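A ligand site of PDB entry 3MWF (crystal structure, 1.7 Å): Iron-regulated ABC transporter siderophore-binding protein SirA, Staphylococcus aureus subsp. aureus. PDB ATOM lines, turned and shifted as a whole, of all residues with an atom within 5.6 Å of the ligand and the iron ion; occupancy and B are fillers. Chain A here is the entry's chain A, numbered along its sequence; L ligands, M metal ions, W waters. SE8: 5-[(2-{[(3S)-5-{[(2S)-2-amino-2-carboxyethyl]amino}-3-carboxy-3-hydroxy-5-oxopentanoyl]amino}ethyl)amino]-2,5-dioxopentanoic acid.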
ATOM      1  N   TRP A  49      21.066 -21.146  30.196  1.00  0.00           N
ATOM      2  CA  TRP A  49      20.765 -19.762  29.960  1.00  0.00           C
ATOM      3  C   TRP A  49      19.396 -19.354  30.508  1.00  0.00           C
ATOM      4  O   TRP A  49      19.199 -18.204  30.941  1.00  0.00           O
ATOM      5  CB  TRP A  49      20.735 -19.484  28.450  1.00  0.00           C
ATOM      6  CG  TRP A  49      22.072 -19.464  27.761  1.00  0.00           C
ATOM      7  CD1 TRP A  49      22.496 -20.324  26.791  1.00  0.00           C
ATOM      8  CD2 TRP A  49      23.127 -18.510  27.953  1.00  0.00           C
ATOM      9  NE1 TRP A  49      23.789 -19.996  26.385  1.00  0.00           N
ATOM     10  CE2 TRP A  49      24.176 -18.871  27.056  1.00  0.00           C
ATOM     11  CE3 TRP A  49      23.278 -17.390  28.765  1.00  0.00           C
ATOM     12  CZ2 TRP A  49      25.385 -18.141  26.961  1.00  0.00           C
ATOM     13  CZ3 TRP A  49      24.490 -16.657  28.692  1.00  0.00           C
ATOM     14  CH2 TRP A  49      25.522 -17.040  27.778  1.00  0.00           C
ATOM     15  N   PRO A  72      29.261 -16.864  30.107  1.00  0.00           N
ATOM     16  CA  PRO A  72      30.186 -15.800  29.707  1.00  0.00           C
ATOM     17  C   PRO A  72      31.426 -15.652  30.597  1.00  0.00           C
ATOM     18  O   PRO A  72      32.395 -15.011  30.186  1.00  0.00           O
ATOM     19  CB  PRO A  72      29.349 -14.535  29.840  1.00  0.00           C
ATOM     20  CG  PRO A  72      27.948 -15.032  29.565  1.00  0.00           C
ATOM     21  CD  PRO A  72      27.895 -16.334  30.290  1.00  0.00           C
ATOM     22  N   VAL A  92      35.237 -18.671  21.712  1.00  0.00           N
ATOM     23  CA  VAL A  92      34.363 -17.526  21.876  1.00  0.00           C
ATOM     24  C   VAL A  92      34.127 -17.118  23.355  1.00  0.00           C
ATOM     25  O   VAL A  92      34.136 -15.931  23.683  1.00  0.00           O
ATOM     26  CB  VAL A  92      33.055 -17.671  21.072  1.00  0.00           C
ATOM     27  CG1 VAL A  92      32.190 -18.806  21.598  1.00  0.00           C
ATOM     28  CG2 VAL A  92      32.316 -16.348  21.102  1.00  0.00           C
ATOM     29  N   ARG A  93      33.924 -18.089  24.241  1.00  0.00           N
ATOM     30  CA  ARG A  93      33.689 -17.743  25.641  1.00  0.00           C
ATOM     31  C   ARG A  93      34.977 -17.609  26.450  1.00  0.00           C
ATOM     32  O   ARG A  93      35.056 -16.753  27.324  1.00  0.00           O
ATOM     33  CB  ARG A  93      32.826 -18.795  26.342  1.00  0.00           C
ATOM     34  CG  ARG A  93      31.474 -19.093  25.648  1.00  0.00           C
ATOM     35  CD  ARG A  93      30.632 -17.873  25.515  1.00  0.00           C
ATOM     36  NE  ARG A  93      29.332 -18.278  24.994  1.00  0.00           N
ATOM     37  CZ  ARG A  93      28.465 -17.450  24.426  1.00  0.00           C
ATOM     38  NH1 ARG A  93      28.765 -16.174  24.271  1.00  0.00           N
ATOM     39  NH2 ARG A  93      27.291 -17.925  24.009  1.00  0.00           N
ATOM     40  N   THR A 112      33.508 -22.139  18.421  1.00  0.00           N
ATOM     41  CA  THR A 112      32.301 -21.525  18.990  1.00  0.00           C
ATOM     42  C   THR A 112      31.423 -22.564  19.676  1.00  0.00           C
ATOM     43  O   THR A 112      31.844 -23.686  19.926  1.00  0.00           O
ATOM     44  CB  THR A 112      31.491 -20.714  17.957  1.00  0.00           C
ATOM     45  OG1 THR A 112      30.451 -19.898  18.611  1.00  0.00           O
ATOM     46  CG2 THR A 112      30.903 -21.668  16.939  1.00  0.00           C
ATOM     47  N   VAL A 113      30.196 -22.154  19.973  1.00  0.00           N
ATOM     48  CA  VAL A 113      29.373 -22.939  20.884  1.00  0.00           C
ATOM     49  C   VAL A 113      28.260 -23.701  20.169  1.00  0.00           C
ATOM     50  O   VAL A 113      27.589 -24.504  20.799  1.00  0.00           O
ATOM     51  CB  VAL A 113      28.753 -22.060  22.008  1.00  0.00           C
ATOM     52  CG1 VAL A 113      29.848 -21.368  22.827  1.00  0.00           C
ATOM     53  CG2 VAL A 113      27.728 -21.024  21.411  1.00  0.00           C
ATOM     54  N   PHE A 114      28.029 -23.379  18.897  1.00  0.00           N
ATOM     55  CA  PHE A 114      26.802 -23.868  18.234  1.00  0.00           C
ATOM     56  C   PHE A 114      27.045 -24.907  17.146  1.00  0.00           C
ATOM     57  O   PHE A 114      26.060 -25.460  16.589  1.00  0.00           O
ATOM     58  CB  PHE A 114      25.950 -22.699  17.677  1.00  0.00           C
ATOM     59  CG  PHE A 114      26.687 -21.804  16.730  1.00  0.00           C
ATOM     60  CD1 PHE A 114      26.993 -22.241  15.415  1.00  0.00           C
ATOM     61  CD2 PHE A 114      27.105 -20.534  17.129  1.00  0.00           C
ATOM     62  CE1 PHE A 114      27.716 -21.406  14.542  1.00  0.00           C
ATOM     63  CE2 PHE A 114      27.793 -19.681  16.290  1.00  0.00           C
ATOM     64  CZ  PHE A 114      28.101 -20.108  14.956  1.00  0.00           C
ATOM     65  N   ARG A 169      14.966  -9.635  20.441  1.00  0.00           N
ATOM     66  CA  ARG A 169      15.650  -9.498  21.754  1.00  0.00           C
ATOM     67  C   ARG A 169      15.087  -8.278  22.443  1.00  0.00           C
ATOM     68  O   ARG A 169      14.157  -7.651  21.944  1.00  0.00           O
ATOM     69  CB  ARG A 169      17.151  -9.360  21.560  1.00  0.00           C
ATOM     70  CG  ARG A 169      17.796 -10.579  20.875  1.00  0.00           C
ATOM     71  CD  ARG A 169      19.111 -10.999  21.594  1.00  0.00           C
ATOM     72  NE  ARG A 169      19.329 -12.411  21.334  1.00  0.00           N
ATOM     73  CZ  ARG A 169      19.885 -13.277  22.143  1.00  0.00           C
ATOM     74  NH1 ARG A 169      20.325 -12.925  23.383  1.00  0.00           N
ATOM     75  NH2 ARG A 169      19.980 -14.506  21.717  1.00  0.00           N
ATOM     76  N   ARG A 174      17.812 -10.060  15.818  1.00  0.00           N
ATOM     77  CA  ARG A 174      18.881 -10.806  15.136  1.00  0.00           C
ATOM     78  C   ARG A 174      18.353 -11.700  14.015  1.00  0.00           C
ATOM     79  O   ARG A 174      17.215 -12.143  14.049  1.00  0.00           O
ATOM     80  CB  ARG A 174      19.633 -11.686  16.137  1.00  0.00           C
ATOM     81  CG  ARG A 174      20.474 -10.846  17.134  1.00  0.00           C
ATOM     82  CD  ARG A 174      21.061 -11.804  18.154  1.00  0.00           C
ATOM     83  NE  ARG A 174      21.827 -11.050  19.165  1.00  0.00           N
ATOM     84  CZ  ARG A 174      22.707 -11.646  19.975  1.00  0.00           C
ATOM     85  NH1 ARG A 174      22.865 -12.971  19.924  1.00  0.00           N
ATOM     86  NH2 ARG A 174      23.386 -10.903  20.867  1.00  0.00           N
ATOM     87  N   TYR A 176      19.544 -15.372  12.673  1.00  0.00           N
ATOM     88  CA  TYR A 176      20.486 -16.476  12.844  1.00  0.00           C
ATOM     89  C   TYR A 176      20.617 -17.117  11.473  1.00  0.00           C
ATOM     90  O   TYR A 176      19.982 -18.121  11.189  1.00  0.00           O
ATOM     91  CB  TYR A 176      20.024 -17.471  13.935  1.00  0.00           C
ATOM     92  CG  TYR A 176      20.308 -16.921  15.303  1.00  0.00           C
ATOM     93  CD1 TYR A 176      19.587 -15.837  15.799  1.00  0.00           C
ATOM     94  CD2 TYR A 176      21.335 -17.483  16.084  1.00  0.00           C
ATOM     95  CE1 TYR A 176      19.888 -15.275  17.058  1.00  0.00           C
ATOM     96  CE2 TYR A 176      21.637 -16.944  17.342  1.00  0.00           C
ATOM     97  CZ  TYR A 176      20.912 -15.841  17.817  1.00  0.00           C
ATOM     98  OH  TYR A 176      21.187 -15.273  19.038  1.00  0.00           O
ATOM     99  N   TYR A 180      23.276 -21.634  15.483  1.00  0.00           N
ATOM    100  CA  TYR A 180      22.763 -22.974  15.739  1.00  0.00           C
ATOM    101  C   TYR A 180      21.691 -23.392  14.740  1.00  0.00           C
ATOM    102  O   TYR A 180      21.849 -24.445  14.074  1.00  0.00           O
ATOM    103  CB  TYR A 180      22.178 -23.072  17.159  1.00  0.00           C
ATOM    104  CG  TYR A 180      21.826 -24.501  17.485  1.00  0.00           C
ATOM    105  CD1 TYR A 180      22.839 -25.444  17.742  1.00  0.00           C
ATOM    106  CD2 TYR A 180      20.481 -24.911  17.505  1.00  0.00           C
ATOM    107  CE1 TYR A 180      22.513 -26.760  18.012  1.00  0.00           C
ATOM    108  CE2 TYR A 180      20.161 -26.258  17.774  1.00  0.00           C
ATOM    109  CZ  TYR A 180      21.174 -27.156  18.023  1.00  0.00           C
ATOM    110  OH  TYR A 180      20.889 -28.458  18.327  1.00  0.00           O
ATOM    111  N   ASP A 205      27.575 -15.026  10.853  1.00  0.00           N
ATOM    112  CA  ASP A 205      26.743 -16.148  11.327  1.00  0.00           C
ATOM    113  C   ASP A 205      25.441 -15.562  11.908  1.00  0.00           C
ATOM    114  O   ASP A 205      24.319 -15.970  11.543  1.00  0.00           O
ATOM    115  CB  ASP A 205      27.407 -16.904  12.490  1.00  0.00           C
ATOM    116  CG  ASP A 205      28.754 -17.538  12.147  1.00  0.00           C
ATOM    117  OD1 ASP A 205      28.876 -18.260  11.122  1.00  0.00           O
ATOM    118  OD2 ASP A 205      29.688 -17.358  12.962  1.00  0.00           O
ATOM    119  N   ILE A 206      25.584 -14.611  12.819  1.00  0.00           N
ATOM    120  CA  ILE A 206      24.437 -14.066  13.546  1.00  0.00           C
ATOM    121  C   ILE A 206      24.471 -12.579  13.279  1.00  0.00           C
ATOM    122  O   ILE A 206      25.471 -11.920  13.609  1.00  0.00           O
ATOM    123  CB  ILE A 206      24.573 -14.365  15.064  1.00  0.00           C
ATOM    124  CG1 ILE A 206      24.550 -15.884  15.279  1.00  0.00           C
ATOM    125  CG2 ILE A 206      23.433 -13.639  15.849  1.00  0.00           C
ATOM    126  CD1 ILE A 206      25.065 -16.374  16.640  1.00  0.00           C
ATOM    127  N   GLN A 208      23.163  -8.849  13.831  1.00  0.00           N
ATOM    128  CA  GLN A 208      22.427  -8.005  14.752  1.00  0.00           C
ATOM    129  C   GLN A 208      21.876  -6.873  13.934  1.00  0.00           C
ATOM    130  O   GLN A 208      22.615  -6.287  13.118  1.00  0.00           O
ATOM    131  CB  GLN A 208      23.344  -7.448  15.832  1.00  0.00           C
ATOM    132  CG  GLN A 208      23.861  -8.514  16.709  1.00  0.00           C
ATOM    133  CD  GLN A 208      24.356  -7.964  18.053  1.00  0.00           C
ATOM    134  OE1 GLN A 208      24.537  -8.730  18.983  1.00  0.00           O
ATOM    135  NE2 GLN A 208      24.557  -6.620  18.147  1.00  0.00           N
ATOM    136  N   SER A 228      13.841 -14.508  22.459  1.00  0.00           N
ATOM    137  CA  SER A 228      14.906 -14.973  23.353  1.00  0.00           C
ATOM    138  C   SER A 228      15.877 -13.861  23.669  1.00  0.00           C
ATOM    139  O   SER A 228      16.411 -13.225  22.768  1.00  0.00           O
ATOM    140  CB  SER A 228      15.647 -16.158  22.719  1.00  0.00           C
ATOM    141  OG  SER A 228      16.673 -16.659  23.578  1.00  0.00           O
ATOM    142  N   ASP A 229      16.079 -13.603  24.959  1.00  0.00           N
ATOM    143  CA  ASP A 229      17.141 -12.706  25.409  1.00  0.00           C
ATOM    144  C   ASP A 229      17.427 -13.052  26.882  1.00  0.00           C
ATOM    145  O   ASP A 229      16.858 -12.413  27.803  1.00  0.00           O
ATOM    146  CB  ASP A 229      16.757 -11.227  25.220  1.00  0.00           C
ATOM    147  CG  ASP A 229      17.923 -10.268  25.433  1.00  0.00           C
ATOM    148  OD1 ASP A 229      18.946 -10.675  26.028  1.00  0.00           O
ATOM    149  OD2 ASP A 229      17.830  -9.078  25.054  1.00  0.00           O
ATOM    150  N   PRO A 230      18.272 -14.079  27.105  1.00  0.00           N
ATOM    151  CA  PRO A 230      18.361 -14.670  28.439  1.00  0.00           C
ATOM    152  C   PRO A 230      18.770 -13.708  29.510  1.00  0.00           C
ATOM    153  O   PRO A 230      18.264 -13.784  30.653  1.00  0.00           O
ATOM    154  CB  PRO A 230      19.468 -15.720  28.276  1.00  0.00           C
ATOM    155  CG  PRO A 230      19.192 -16.235  26.861  1.00  0.00           C
ATOM    156  CD  PRO A 230      18.887 -14.942  26.074  1.00  0.00           C
ATOM    157  N   ASN A 231      19.692 -12.824  29.179  1.00  0.00           N
ATOM    158  CA  ASN A 231      20.194 -11.906  30.190  1.00  0.00           C
ATOM    159  C   ASN A 231      19.505 -10.536  30.311  1.00  0.00           C
ATOM    160  O   ASN A 231      19.918  -9.683  31.125  1.00  0.00           O
ATOM    161  CB  ASN A 231      21.700 -11.839  30.064  1.00  0.00           C
ATOM    162  CG  ASN A 231      22.359 -13.102  30.642  1.00  0.00           C
ATOM    163  OD1 ASN A 231      23.540 -13.371  30.416  1.00  0.00           O
ATOM    164  ND2 ASN A 231      21.585 -13.871  31.411  1.00  0.00           N
ATOM    165  N   ASN A 272      17.869 -22.470  19.874  1.00  0.00           N
ATOM    166  CA  ASN A 272      19.152 -21.796  20.014  1.00  0.00           C
ATOM    167  C   ASN A 272      19.942 -22.085  21.282  1.00  0.00           C
ATOM    168  O   ASN A 272      21.184 -22.227  21.231  1.00  0.00           O
ATOM    169  CB  ASN A 272      18.968 -20.267  19.929  1.00  0.00           C
ATOM    170  CG  ASN A 272      20.305 -19.562  19.785  1.00  0.00           C
ATOM    171  OD1 ASN A 272      21.094 -19.916  18.898  1.00  0.00           O
ATOM    172  ND2 ASN A 272      20.557 -18.577  20.636  1.00  0.00           N
ATOM    173  N   LEU A 273      19.259 -22.122  22.419  1.00  0.00           N
ATOM    174  CA  LEU A 273      20.046 -22.070  23.682  1.00  0.00           C
ATOM    175  C   LEU A 273      20.785 -23.340  24.032  1.00  0.00           C
ATOM    176  O   LEU A 273      21.911 -23.251  24.540  1.00  0.00           O
ATOM    177  CB  LEU A 273      19.175 -21.622  24.867  1.00  0.00           C
ATOM    178  CG  LEU A 273      18.520 -20.243  24.727  1.00  0.00           C
ATOM    179  CD1 LEU A 273      17.633 -19.939  25.958  1.00  0.00           C
ATOM    180  CD2 LEU A 273      19.490 -19.054  24.444  1.00  0.00           C
HETATM  181  C1  SE8 L   1      25.568 -13.836  25.796  1.00  0.00           C
HETATM  182  C2  SE8 L   1      24.130 -13.494  25.546  1.00  0.00           C
HETATM  183  C3  SE8 L   1      23.207 -14.568  26.102  1.00  0.00           C
HETATM  184  N4  SE8 L   1      23.335 -15.845  25.410  1.00  0.00           N
HETATM  185  C5  SE8 L   1      22.552 -16.173  24.397  1.00  0.00           C
HETATM  186  C6  SE8 L   1      22.896 -17.439  23.653  1.00  0.00           C
HETATM  187  C7  SE8 L   1      23.962 -17.173  22.592  1.00  0.00           C
HETATM  188  C8  SE8 L   1      24.390 -18.528  22.001  1.00  0.00           C
HETATM  189  C9  SE8 L   1      25.292 -18.423  20.776  1.00  0.00           C
HETATM  190  N10 SE8 L   1      26.171 -17.425  20.733  1.00  0.00           N
HETATM  191  C11 SE8 L   1      27.056 -17.335  19.586  1.00  0.00           C
HETATM  192  C12 SE8 L   1      28.504 -17.451  20.023  1.00  0.00           C
HETATM  193  N13 SE8 L   1      29.427 -16.928  19.016  1.00  0.00           N
HETATM  194  C14 SE8 L   1      29.740 -15.608  18.888  1.00  0.00           C
HETATM  195  C15 SE8 L   1      29.486 -14.663  20.029  1.00  0.00           C
HETATM  196  C16 SE8 L   1      28.016 -14.365  19.882  1.00  0.00           C
HETATM  197  C17 SE8 L   1      27.278 -14.100  21.163  1.00  0.00           C
HETATM  198  C18 SE8 L   1      26.576 -12.827  21.168  1.00  0.00           C
HETATM  199  O19 SE8 L   1      26.027 -13.721  26.959  1.00  0.00           O
HETATM  200  O20 SE8 L   1      26.267 -14.190  24.820  1.00  0.00           O
HETATM  201  N21 SE8 L   1      23.922 -13.321  24.102  1.00  0.00           N
HETATM  202  O22 SE8 L   1      21.592 -15.518  24.049  1.00  0.00           O
HETATM  203  C23 SE8 L   1      23.433 -16.218  21.547  1.00  0.00           C
HETATM  204  O24 SE8 L   1      22.623 -16.642  20.675  1.00  0.00           O
HETATM  205  O25 SE8 L   1      23.816 -15.023  21.534  1.00  0.00           O
HETATM  206  O26 SE8 L   1      25.072 -16.499  23.216  1.00  0.00           O
HETATM  207  O27 SE8 L   1      25.193 -19.257  19.887  1.00  0.00           O
HETATM  208  O28 SE8 L   1      30.205 -15.133  17.860  1.00  0.00           O
HETATM  209  O29 SE8 L   1      27.151 -14.936  22.060  1.00  0.00           O
HETATM  210  O30 SE8 L   1      25.599 -12.703  21.899  1.00  0.00           O
HETATM  211  O31 SE8 L   1      26.948 -11.890  20.411  1.00  0.00           O
HETATM  212 FE    FE M   1      25.339 -14.563  22.948  1.00  0.00          FE
HETATM  213  O   HOH W   1      23.515 -19.701  17.575  1.00  0.00           O
HETATM  214  O   HOH W   2      23.796 -21.798  20.408  1.00  0.00           O
HETATM  215  O   HOH W   3      25.402 -10.999  18.130  1.00  0.00           O
HETATM  216  O   HOH W   4      24.256 -10.176  24.170  1.00  0.00           O
HETATM  217  O   HOH W   5      20.857 -12.138  26.626  1.00  0.00           O
HETATM  218  O   HOH W   6      25.657 -20.627  24.439  1.00  0.00           O
HETATM  219  O   HOH W   7      28.653 -12.984  26.604  1.00  0.00           O
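The iron ion is bound by O26 of the ligand (2.0 Å), O29 of the ligand (2.1 Å), O20 of the ligand (2.1 Å), O25 of the ligand (2.1 Å), O30 of the ligand (2.2 Å) and N21 of the ligand (2.2 Å).
No residue comes within 4 Å of the iron ion. The nearest printed residue that does not touch the iron ion is Arg 93 (4.01 Å).
The backbone carbonyl oxygen of Ser 228 is in hydrogen-bond range of the guanidinium group of Arg 169, at 3.4 Å. The guanidinium group (NH2) of Arg 174 is in hydrogen-bond range of the side-chain amide oxygen (OE1) of Gln 208. The side-chain hydroxyl of Tyr 176 lies within hydrogen-bond range of the guanidinium group of Arg 174, at 3.0 Å. The side-chain hydroxyl of Tyr 176 lies within hydrogen-bond range of the guanidinium group of Arg 169, at 3.0 Å. NH1 of Arg 169 is in salt-bridge range of OD1 of Asp 229, 3.7 Å away.
OG1 of Thr 112 lies within hydrogen-bond range of N13 of the ligand (3.2 Å). NH2 of Arg 169 is in salt-bridge range of O24 of the ligand (3.6 Å). NH2 of Arg 174 is in salt-bridge range of O31 of the ligand, at 3.7 Å. ND2 of Asn 272 lies within hydrogen-bond range of O24 of the ligand (2.8 Å). The side-chain hydroxyl (OH) of Tyr 176 lies within hydrogen-bond range of an oxygen (O24) of the ligand, 2.6 Å away. NH2 of Arg 93 sits close to O26 of the ligand, 2.8 Å away.
Water W1 lies within hydrogen-bond range of OD1 of Asn 272 (2.8 Å), N of Tyr 180 (2.9 Å) and O27 of the ligand (2.9 Å). Water W3 lies within hydrogen-bond range of the side-chain amide oxygen (OE1) of Gln 208 (2.6 Å), an oxygen (O31) of the ligand (2.9 Å) and the guanidinium group (NH2) of Arg 174 (3.4 Å). Water W2 bridges the backbone carbonyl oxygen (O) of Asn 272 (2.8 Å) and an oxygen (O27) of the ligand (2.9 Å). Water W5 lies within hydrogen-bond range of the side-chain carboxylate (OD1) of Asp 229 (2.5 Å), the backbone NH (N) of Asn 231 (2.9 Å) and the guanidinium group (NH1) of Arg 169 (3.4 Å). Water W6 bridges the indole nitrogen of Trp 49 (2.8 Å) and the guanidinium group of Arg 93 (3.2 Å).
Residues that only touch the ligand: Trp 49, Pro 72, Val 92, Val 113, Phe 114, Ile 206, Pro 230 and Leu 273. Hydrophobic or aromatic side chains that line the ligand: Trp 49, Pro 72, Val 92, Val 113, Phe 114, Tyr 176, Ile 206, Pro 230 and Leu 273. Along chain A the residues within 4 Å of the ligand span positions 49 to 273. The nearest printed residue that does not touch the ligand is Gln 208 (4.2 Å).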
